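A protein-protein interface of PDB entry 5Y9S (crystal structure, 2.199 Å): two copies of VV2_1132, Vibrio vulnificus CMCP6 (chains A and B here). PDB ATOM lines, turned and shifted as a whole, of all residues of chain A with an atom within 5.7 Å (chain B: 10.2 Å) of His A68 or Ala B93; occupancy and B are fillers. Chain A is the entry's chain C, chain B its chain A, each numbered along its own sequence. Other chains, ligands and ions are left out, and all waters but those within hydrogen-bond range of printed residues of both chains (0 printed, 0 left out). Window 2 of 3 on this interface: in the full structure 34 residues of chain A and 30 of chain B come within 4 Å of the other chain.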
ATOM      1  N   VAL A  53      28.943  26.639  -0.793  1.00  0.00           N
ATOM      2  CA  VAL A  53      29.601  25.406  -0.322  1.00  0.00           C
ATOM      3  C   VAL A  53      30.828  25.104  -1.171  1.00  0.00           C
ATOM      4  O   VAL A  53      30.871  25.509  -2.343  1.00  0.00           O
ATOM      5  CB  VAL A  53      28.665  24.189  -0.368  1.00  0.00           C
ATOM      6  CG1 VAL A  53      27.758  24.166   0.850  1.00  0.00           C
ATOM      7  CG2 VAL A  53      27.886  24.172  -1.664  1.00  0.00           C
ATOM      8  N   PRO A  54      31.836  24.400  -0.650  1.00  0.00           N
ATOM      9  CA  PRO A  54      32.991  24.076  -1.494  1.00  0.00           C
ATOM     10  C   PRO A  54      32.560  23.087  -2.557  1.00  0.00           C
ATOM     11  O   PRO A  54      31.763  22.180  -2.299  1.00  0.00           O
ATOM     12  CB  PRO A  54      34.009  23.467  -0.522  1.00  0.00           C
ATOM     13  CG  PRO A  54      33.170  22.913   0.602  1.00  0.00           C
ATOM     14  CD  PRO A  54      31.960  23.833   0.712  1.00  0.00           C
ATOM     15  N   LEU A  55      33.058  23.298  -3.771  1.00  0.00           N
ATOM     16  CA  LEU A  55      32.692  22.442  -4.886  1.00  0.00           C
ATOM     17  C   LEU A  55      33.758  21.407  -5.206  1.00  0.00           C
ATOM     18  O   LEU A  55      33.447  20.424  -5.899  1.00  0.00           O
ATOM     19  CB  LEU A  55      32.426  23.293  -6.136  1.00  0.00           C
ATOM     20  CG  LEU A  55      31.264  24.270  -5.960  1.00  0.00           C
ATOM     21  CD1 LEU A  55      31.205  25.220  -7.153  1.00  0.00           C
ATOM     22  CD2 LEU A  55      29.953  23.498  -5.806  1.00  0.00           C
ATOM     23  N   THR A  66      33.496  17.727  -4.924  1.00  0.00           N
ATOM     24  CA  THR A  66      32.730  17.369  -3.740  1.00  0.00           C
ATOM     25  C   THR A  66      31.338  16.871  -4.132  1.00  0.00           C
ATOM     26  O   THR A  66      30.928  16.870  -5.298  1.00  0.00           O
ATOM     27  CB  THR A  66      32.622  18.566  -2.793  1.00  0.00           C
ATOM     28  OG1 THR A  66      31.732  19.550  -3.346  1.00  0.00           O
ATOM     29  CG2 THR A  66      34.000  19.171  -2.514  1.00  0.00           C
ATOM     30  N   GLU A  67      30.622  16.407  -3.119  1.00  0.00           N
ATOM     31  CA  GLU A  67      29.203  16.127  -3.253  1.00  0.00           C
ATOM     32  C   GLU A  67      28.467  17.321  -3.868  1.00  0.00           C
ATOM     33  O   GLU A  67      27.681  17.165  -4.807  1.00  0.00           O
ATOM     34  CB  GLU A  67      28.645  15.756  -1.874  1.00  0.00           C
ATOM     35  CG  GLU A  67      29.604  14.856  -1.004  1.00  0.00           C
ATOM     36  CD  GLU A  67      30.930  15.533  -0.507  1.00  0.00           C
ATOM     37  OE1 GLU A  67      32.025  14.938  -0.671  1.00  0.00           O
ATOM     38  OE2 GLU A  67      30.887  16.655   0.041  1.00  0.00           O
ATOM     39  N   HIS A  68      28.754  18.529  -3.395  1.00  0.00           N
ATOM     40  CA  HIS A  68      28.088  19.711  -3.938  1.00  0.00           C
ATOM     41  C   HIS A  68      28.520  20.020  -5.370  1.00  0.00           C
ATOM     42  O   HIS A  68      27.704  20.522  -6.161  1.00  0.00           O
ATOM     43  CB  HIS A  68      28.353  20.902  -3.034  1.00  0.00           C
ATOM     44  CG  HIS A  68      28.003  20.637  -1.602  1.00  0.00           C
ATOM     45  ND1 HIS A  68      28.939  20.645  -0.588  1.00  0.00           N
ATOM     46  CD2 HIS A  68      26.825  20.307  -1.026  1.00  0.00           C
ATOM     47  CE1 HIS A  68      28.344  20.360   0.557  1.00  0.00           C
ATOM     48  NE2 HIS A  68      27.062  20.154   0.320  1.00  0.00           N
ATOM     49  N   GLY A  69      29.793  19.762  -5.710  1.00  0.00           N
ATOM     50  CA  GLY A  69      30.254  19.956  -7.082  1.00  0.00           C
ATOM     51  C   GLY A  69      29.559  19.024  -8.056  1.00  0.00           C
ATOM     52  O   GLY A  69      29.213  19.417  -9.181  1.00  0.00           O
ATOM     53  N   GLN A  70      29.316  17.786  -7.630  1.00  0.00           N
ATOM     54  CA  GLN A  70      28.562  16.861  -8.454  1.00  0.00           C
ATOM     55  C   GLN A  70      27.181  17.421  -8.752  1.00  0.00           C
ATOM     56  O   GLN A  70      26.802  17.592  -9.918  1.00  0.00           O
ATOM     57  CB  GLN A  70      28.475  15.500  -7.765  1.00  0.00           C
ATOM     58  CG  GLN A  70      29.835  14.823  -7.652  1.00  0.00           C
ATOM     59  CD  GLN A  70      29.802  13.580  -6.800  1.00  0.00           C
ATOM     60  OE1 GLN A  70      28.734  13.099  -6.413  1.00  0.00           O
ATOM     61  NE2 GLN A  70      30.983  13.060  -6.482  1.00  0.00           N
ATOM     62  N   LYS A  71      26.432  17.758  -7.696  1.00  0.00           N
ATOM     63  CA  LYS A  71      25.107  18.354  -7.856  1.00  0.00           C
ATOM     64  C   LYS A  71      25.150  19.589  -8.759  1.00  0.00           C
ATOM     65  O   LYS A  71      24.228  19.827  -9.540  1.00  0.00           O
ATOM     66  CB  LYS A  71      24.539  18.701  -6.473  1.00  0.00           C
ATOM     67  CG  LYS A  71      23.076  19.140  -6.420  1.00  0.00           C
ATOM     68  CD  LYS A  71      22.789  19.866  -5.081  1.00  0.00           C
ATOM     69  CE  LYS A  71      21.379  20.491  -5.004  1.00  0.00           C
ATOM     70  NZ  LYS A  71      20.361  19.478  -4.696  1.00  0.00           N
ATOM     71  N   PHE A  72      26.235  20.362  -8.696  1.00  0.00           N
ATOM     72  CA  PHE A  72      26.302  21.631  -9.419  1.00  0.00           C
ATOM     73  C   PHE A  72      26.564  21.483 -10.911  1.00  0.00           C
ATOM     74  O   PHE A  72      26.322  22.430 -11.660  1.00  0.00           O
ATOM     75  CB  PHE A  72      27.392  22.505  -8.812  1.00  0.00           C
ATOM     76  CG  PHE A  72      27.398  23.924  -9.317  1.00  0.00           C
ATOM     77  CD1 PHE A  72      26.464  24.841  -8.865  1.00  0.00           C
ATOM     78  CD2 PHE A  72      28.370  24.355 -10.211  1.00  0.00           C
ATOM     79  CE1 PHE A  72      26.486  26.162  -9.315  1.00  0.00           C
ATOM     80  CE2 PHE A  72      28.400  25.676 -10.651  1.00  0.00           C
ATOM     81  CZ  PHE A  72      27.464  26.576 -10.208  1.00  0.00           C
ATOM     82  N   VAL A  73      27.080  20.353 -11.351  1.00  0.00           N
ATOM     83  CA  VAL A  73      27.428  20.193 -12.766  1.00  0.00           C
ATOM     84  C   VAL A  73      26.268  20.577 -13.683  1.00  0.00           C
ATOM     85  O   VAL A  73      26.471  21.416 -14.572  1.00  0.00           O
ATOM     86  CB  VAL A  73      27.959  18.785 -13.029  1.00  0.00           C
ATOM     87  CG1 VAL A  73      27.971  18.499 -14.535  1.00  0.00           C
ATOM     88  CG2 VAL A  73      29.365  18.628 -12.480  1.00  0.00           C
ATOM     89  N   THR B  86      19.194  28.255  -9.025  1.00  0.00           N
ATOM     90  CA  THR B  86      20.499  27.763  -8.615  1.00  0.00           C
ATOM     91  C   THR B  86      20.784  28.131  -7.166  1.00  0.00           C
ATOM     92  O   THR B  86      21.091  27.265  -6.340  1.00  0.00           O
ATOM     93  CB  THR B  86      21.575  28.329  -9.529  1.00  0.00           C
ATOM     94  OG1 THR B  86      21.359  27.872 -10.867  1.00  0.00           O
ATOM     95  CG2 THR B  86      22.971  27.907  -9.036  1.00  0.00           C
ATOM     96  N   LYS B  87      20.636  29.413  -6.832  1.00  0.00           N
ATOM     97  CA  LYS B  87      20.862  29.857  -5.465  1.00  0.00           C
ATOM     98  C   LYS B  87      19.923  29.152  -4.498  1.00  0.00           C
ATOM     99  O   LYS B  87      20.353  28.677  -3.439  1.00  0.00           O
ATOM    100  CB  LYS B  87      20.711  31.374  -5.392  1.00  0.00           C
ATOM    101  CG  LYS B  87      22.029  32.111  -5.193  1.00  0.00           C
ATOM    102  CD  LYS B  87      22.517  31.861  -3.775  1.00  0.00           C
ATOM    103  CE  LYS B  87      23.879  32.441  -3.504  1.00  0.00           C
ATOM    104  NZ  LYS B  87      23.972  33.928  -3.561  1.00  0.00           N
ATOM    105  N   GLU B  88      18.649  29.010  -4.873  1.00  0.00           N
ATOM    106  CA  GLU B  88      17.691  28.366  -3.977  1.00  0.00           C
ATOM    107  C   GLU B  88      18.055  26.905  -3.735  1.00  0.00           C
ATOM    108  O   GLU B  88      18.143  26.469  -2.588  1.00  0.00           O
ATOM    109  CB  GLU B  88      16.278  28.485  -4.543  1.00  0.00           C
ATOM    110  CG  GLU B  88      15.741  29.890  -4.438  1.00  0.00           C
ATOM    111  CD  GLU B  88      14.456  30.092  -5.211  1.00  0.00           C
ATOM    112  OE1 GLU B  88      13.991  29.137  -5.884  1.00  0.00           O
ATOM    113  OE2 GLU B  88      13.918  31.217  -5.140  1.00  0.00           O
ATOM    114  N   ASP B  89      18.289  26.140  -4.809  1.00  0.00           N
ATOM    115  CA  ASP B  89      18.604  24.717  -4.675  1.00  0.00           C
ATOM    116  C   ASP B  89      19.874  24.462  -3.851  1.00  0.00           C
ATOM    117  O   ASP B  89      20.073  23.338  -3.379  1.00  0.00           O
ATOM    118  CB  ASP B  89      18.717  24.063  -6.069  1.00  0.00           C
ATOM    119  CG  ASP B  89      17.361  23.962  -6.770  1.00  0.00           C
ATOM    120  OD1 ASP B  89      16.372  24.312  -6.111  1.00  0.00           O
ATOM    121  OD2 ASP B  89      17.263  23.558  -7.956  1.00  0.00           O
ATOM    122  N   PHE B  90      20.725  25.465  -3.639  1.00  0.00           N
ATOM    123  CA  PHE B  90      21.928  25.248  -2.847  1.00  0.00           C
ATOM    124  C   PHE B  90      21.897  25.913  -1.475  1.00  0.00           C
ATOM    125  O   PHE B  90      22.830  25.719  -0.693  1.00  0.00           O
ATOM    126  CB  PHE B  90      23.160  25.697  -3.643  1.00  0.00           C
ATOM    127  CG  PHE B  90      23.584  24.678  -4.669  1.00  0.00           C
ATOM    128  CD1 PHE B  90      23.011  24.662  -5.928  1.00  0.00           C
ATOM    129  CD2 PHE B  90      24.502  23.696  -4.347  1.00  0.00           C
ATOM    130  CE1 PHE B  90      23.372  23.701  -6.856  1.00  0.00           C
ATOM    131  CE2 PHE B  90      24.873  22.735  -5.268  1.00  0.00           C
ATOM    132  CZ  PHE B  90      24.308  22.736  -6.523  1.00  0.00           C
ATOM    133  N   ALA B  91      20.842  26.648  -1.138  1.00  0.00           N
ATOM    134  CA  ALA B  91      20.819  27.354   0.136  1.00  0.00           C
ATOM    135  C   ALA B  91      20.956  26.369   1.284  1.00  0.00           C
ATOM    136  O   ALA B  91      20.322  25.310   1.297  1.00  0.00           O
ATOM    137  CB  ALA B  91      19.534  28.161   0.292  1.00  0.00           C
ATOM    138  N   GLN B  92      21.819  26.701   2.236  1.00  0.00           N
ATOM    139  CA  GLN B  92      22.024  25.855   3.401  1.00  0.00           C
ATOM    140  C   GLN B  92      22.519  24.467   3.011  1.00  0.00           C
ATOM    141  O   GLN B  92      22.367  23.512   3.776  1.00  0.00           O
ATOM    142  CB  GLN B  92      20.735  25.755   4.241  1.00  0.00           C
ATOM    143  CG  GLN B  92      20.226  27.102   4.782  1.00  0.00           C
ATOM    144  CD  GLN B  92      19.677  27.005   6.210  1.00  0.00           C
ATOM    145  OE1 GLN B  92      18.897  26.100   6.538  1.00  0.00           O
ATOM    146  NE2 GLN B  92      20.095  27.935   7.066  1.00  0.00           N
ATOM    147  N   ALA B  93      23.116  24.335   1.823  1.00  0.00           N
ATOM    148  CA  ALA B  93      23.736  23.073   1.458  1.00  0.00           C
ATOM    149  C   ALA B  93      24.806  22.669   2.448  1.00  0.00           C
ATOM    150  O   ALA B  93      25.105  21.478   2.570  1.00  0.00           O
ATOM    151  CB  ALA B  93      24.368  23.157   0.070  1.00  0.00           C
ATOM    152  N   SER B  94      25.432  23.639   3.124  1.00  0.00           N
ATOM    153  CA  SER B  94      26.467  23.301   4.099  1.00  0.00           C
ATOM    154  C   SER B  94      25.888  22.778   5.401  1.00  0.00           C
ATOM    155  O   SER B  94      26.584  22.057   6.130  1.00  0.00           O
ATOM    156  CB  SER B  94      27.367  24.508   4.400  1.00  0.00           C
ATOM    157  OG  SER B  94      26.646  25.727   4.455  1.00  0.00           O
ATOM    158  N   LEU B  95      24.625  23.094   5.689  1.00  0.00           N
ATOM    159  CA  LEU B  95      24.030  22.777   6.983  1.00  0.00           C
ATOM    160  C   LEU B  95      23.695  21.293   7.035  1.00  0.00           C
ATOM    161  O   LEU B  95      22.734  20.843   6.407  1.00  0.00           O
ATOM    162  CB  LEU B  95      22.796  23.636   7.225  1.00  0.00           C
ATOM    163  CG  LEU B  95      22.213  23.495   8.632  1.00  0.00           C
ATOM    164  CD1 LEU B  95      23.230  23.920   9.696  1.00  0.00           C
ATOM    165  CD2 LEU B  95      20.910  24.289   8.758  1.00  0.00           C
ATOM    166  N   LYS B  96      24.487  20.539   7.798  1.00  0.00           N
ATOM    167  CA  LYS B  96      24.305  19.095   7.904  1.00  0.00           C
ATOM    168  C   LYS B  96      23.083  18.761   8.752  1.00  0.00           C
ATOM    169  O   LYS B  96      22.118  18.163   8.264  1.00  0.00           O
ATOM    170  CB  LYS B  96      25.564  18.451   8.502  1.00  0.00           C
ATOM    171  CG  LYS B  96      26.741  18.293   7.537  1.00  0.00           C
ATOM    172  CD  LYS B  96      28.015  17.810   8.256  1.00  0.00           C
ATOM    173  CE  LYS B  96      29.009  18.950   8.501  1.00  0.00           C
ATOM    174  NZ  LYS B  96      29.325  19.685   7.240  1.00  0.00           N
ATOM    175  N   THR B  97      23.113  19.127  10.028  1.00  0.00           N
ATOM    176  CA  THR B  97      22.013  18.892  10.954  1.00  0.00           C
ATOM    177  C   THR B  97      21.370  20.213  11.340  1.00  0.00           C
ATOM    178  O   THR B  97      21.907  21.292  11.099  1.00  0.00           O
ATOM    179  CB  THR B  97      22.489  18.192  12.231  1.00  0.00           C
ATOM    180  OG1 THR B  97      22.971  19.180  13.154  1.00  0.00           O
ATOM    181  CG2 THR B  97      23.586  17.190  11.931  1.00  0.00           C
ATOM    182  N   THR B 100      23.282  22.358  14.230  1.00  0.00           N
ATOM    183  CA  THR B 100      24.655  22.697  13.874  1.00  0.00           C
ATOM    184  C   THR B 100      24.791  24.208  13.721  1.00  0.00           C
ATOM    185  O   THR B 100      24.015  24.841  12.999  1.00  0.00           O
ATOM    186  CB  THR B 100      25.097  21.984  12.586  1.00  0.00           C
ATOM    187  OG1 THR B 100      25.453  20.628  12.883  1.00  0.00           O
ATOM    188  CG2 THR B 100      26.321  22.661  11.989  1.00  0.00           C
ATOM    189  N   ARG B 102      27.309  26.807  12.228  1.00  0.00           N
ATOM    190  CA  ARG B 102      28.452  26.987  11.345  1.00  0.00           C
ATOM    191  C   ARG B 102      29.180  28.278  11.693  1.00  0.00           C
ATOM    192  O   ARG B 102      28.602  29.368  11.619  1.00  0.00           O
ATOM    193  CB  ARG B 102      27.981  27.018   9.897  1.00  0.00           C
ATOM    194  CG  ARG B 102      27.212  25.807   9.480  1.00  0.00           C
ATOM    195  CD  ARG B 102      26.463  26.097   8.216  1.00  0.00           C
ATOM    196  NE  ARG B 102      25.392  27.050   8.452  1.00  0.00           N
ATOM    197  CZ  ARG B 102      24.496  27.398   7.538  1.00  0.00           C
ATOM    198  NH1 ARG B 102      24.553  26.872   6.328  1.00  0.00           N
ATOM    199  NH2 ARG B 102      23.548  28.277   7.838  1.00  0.00           N
ATOM    200  N   MET B 145      28.594  35.559   2.948  1.00  0.00           N
ATOM    201  CA  MET B 145      28.082  34.252   3.352  1.00  0.00           C
ATOM    202  C   MET B 145      27.126  34.356   4.533  1.00  0.00           C
ATOM    203  O   MET B 145      26.225  33.519   4.668  1.00  0.00           O
ATOM    204  CB  MET B 145      29.219  33.292   3.699  1.00  0.00           C
ATOM    205  CG  MET B 145      30.359  33.287   2.752  1.00  0.00           C
ATOM    206  SD  MET B 145      31.601  32.094   3.257  1.00  0.00           S
ATOM    207  CE  MET B 145      31.119  30.637   2.382  1.00  0.00           C
ATOM    208  N   ASP B 148      23.801  35.356   2.933  1.00  0.00           N
ATOM    209  CA  ASP B 148      23.230  34.208   2.239  1.00  0.00           C
ATOM    210  C   ASP B 148      22.825  33.090   3.180  1.00  0.00           C
ATOM    211  O   ASP B 148      22.176  32.140   2.725  1.00  0.00           O
ATOM    212  CB  ASP B 148      24.218  33.659   1.201  1.00  0.00           C
ATOM    213  CG  ASP B 148      24.544  34.671   0.117  1.00  0.00           C
ATOM    214  OD1 ASP B 148      23.657  35.487  -0.211  1.00  0.00           O
ATOM    215  OD2 ASP B 148      25.674  34.642  -0.428  1.00  0.00           O
ATOM    216  N   HIS B 149      23.186  33.166   4.463  1.00  0.00           N
ATOM    217  CA  HIS B 149      22.956  32.067   5.405  1.00  0.00           C
ATOM    218  C   HIS B 149      23.796  30.841   5.063  1.00  0.00           C
ATOM    219  O   HIS B 149      23.415  29.709   5.371  1.00  0.00           O
ATOM    220  CB  HIS B 149      21.478  31.648   5.485  1.00  0.00           C
ATOM    221  CG  HIS B 149      20.540  32.744   5.882  1.00  0.00           C
ATOM    222  ND1 HIS B 149      20.955  34.030   6.148  1.00  0.00           N
ATOM    223  CD2 HIS B 149      19.199  32.734   6.064  1.00  0.00           C
ATOM    224  CE1 HIS B 149      19.910  34.768   6.478  1.00  0.00           C
ATOM    225  NE2 HIS B 149      18.833  34.005   6.435  1.00  0.00           N
ATOM    226  N   SER B 150      24.934  31.057   4.402  1.00  0.00           N
ATOM    227  CA  SER B 150      25.896  29.995   4.131  1.00  0.00           C
ATOM    228  C   SER B 150      26.737  29.661   5.352  1.00  0.00           C
ATOM    229  O   SER B 150      27.250  28.539   5.451  1.00  0.00           O
ATOM    230  CB  SER B 150      26.810  30.405   2.976  1.00  0.00           C
ATOM    231  OG  SER B 150      26.091  30.354   1.767  1.00  0.00           O
ATOM    232  N   THR B 151      26.895  30.621   6.264  1.00  0.00           N
ATOM    233  CA  THR B 151      27.416  30.382   7.596  1.00  0.00           C
ATOM    234  C   THR B 151      26.489  31.054   8.611  1.00  0.00           C
ATOM    235  O   THR B 151      25.541  31.753   8.252  1.00  0.00           O
ATOM    236  CB  THR B 151      28.860  30.885   7.729  1.00  0.00           C
ATOM    237  OG1 THR B 151      29.447  30.302   8.895  1.00  0.00           O
ATOM    238  CG2 THR B 151      28.902  32.406   7.856  1.00  0.00           C
ATOM    239  N   ASP B 152      26.751  30.820   9.888  1.00  0.00           N
ATOM    240  CA  ASP B 152      25.918  31.347  10.964  1.00  0.00           C
ATOM    241  C   ASP B 152      26.572  32.450  11.777  1.00  0.00           C
ATOM    242  O   ASP B 152      25.920  33.451  12.084  1.00  0.00           O
ATOM    243  CB  ASP B 152      25.514  30.207  11.883  1.00  0.00           C
ATOM    244  CG  ASP B 152      24.827  29.104  11.125  1.00  0.00           C
ATOM    245  OD1 ASP B 152      24.024  29.446  10.229  1.00  0.00           O
ATOM    246  OD2 ASP B 152      25.094  27.915  11.401  1.00  0.00           O
ATOM    247  N   ARG B 291      17.162  30.865  12.826  1.00  0.00           N
ATOM    248  CA  ARG B 291      17.183  29.488  13.301  1.00  0.00           C
ATOM    249  C   ARG B 291      17.468  29.460  14.797  1.00  0.00           C
ATOM    250  O   ARG B 291      18.256  30.260  15.314  1.00  0.00           O
ATOM    251  CB  ARG B 291      18.224  28.657  12.547  1.00  0.00           C
ATOM    252  CG  ARG B 291      18.164  27.164  12.894  1.00  0.00           C
ATOM    253  CD  ARG B 291      18.754  26.289  11.804  1.00  0.00           C
ATOM    254  NE  ARG B 291      20.164  26.038  12.048  1.00  0.00           N
ATOM    255  CZ  ARG B 291      21.123  26.773  11.514  1.00  0.00           C
ATOM    256  NH1 ARG B 291      20.802  27.771  10.699  1.00  0.00           N
ATOM    257  NH2 ARG B 291      22.389  26.502  11.775  1.00  0.00           N
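Ala B93 touches Val A53 (CB to CG1, 3.6 Å). CG1 of Val A53 touches N of Ser B94, 3.3 Å away. O of His A68 touches CE2 of Phe B90, 3.7 Å away. Asp B89 touches Lys A71. Phe B90 touches Lys A71 (CE2 to CD, 3.6 Å). Phe A72 touches Thr B86 (CE1 to CG2, 3.9 Å). CZ of Phe B90 touches CA of Phe A72, at 3.7 Å.
The backbone carbonyl oxygen of Ala B93 lies within hydrogen-bond range of a ring nitrogen (NE2) of His A68, 3.3 Å away.
No position is printed for both chains. Of the 8 pairs that touch across the chains among the printed residues, none has its exchanged pair printed and touching as well.
Of the 11 printed residues of chain A, 4 touch a printed residue of chain B. Hydrophobic or aromatic side chains of chain A that line the printed part of chain B: Val A53, His A68 and Phe A72. Along chain A the printed residues that touch a printed residue of chain B span positions 53 to 72. Hydrophobic or aromatic side chains of chain B within 4 Å of the printed part of chain A: Phe B90 and Ala B93. Among the printed residues, no Asp or Glu carboxylate lies within 4 Å of a Lys or Arg side-chain nitrogen of the other chain.
The guanidinium group (NH1) of Arg B102 sits at hydrogen-bond distance from the side-chain hydroxyl (OG) of Ser B94, 3.0 Å away. OG of Ser B94 is in hydrogen-bond range of O of Ser B150, at 3.0 Å. The side-chain hydroxyl (OG1) of Thr A66 sits at hydrogen-bond distance from the backbone NH (N) of His A68.
Ala B93 touches two residues of chain A. No residue of chain B comes within 4 Å of Leu A55. No residue of chain B comes within 4 Å of Gly A69. Of the printed residues of chain A, Ser B94 touches Val A53. Of the printed residues of chain A, Phe B90 touches His A68, Lys A71 and Phe A72. Of the printed residues of chain B, Lys A71 touches Asp B89 (3.5 Å) and Phe B90 (3.6 Å). Of the printed residues of chain A, Thr B86 touches Phe A72 (3.9 Å). Of the printed residues of chain A, Asp B89 touches Lys A71. Asp B148 touches none of the printed residues of chain A. Lys B96 touches none of the printed residues of chain A. The nearest printed residue of chain A that does not touch Phe B90 is Val A53 (4.3 Å).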
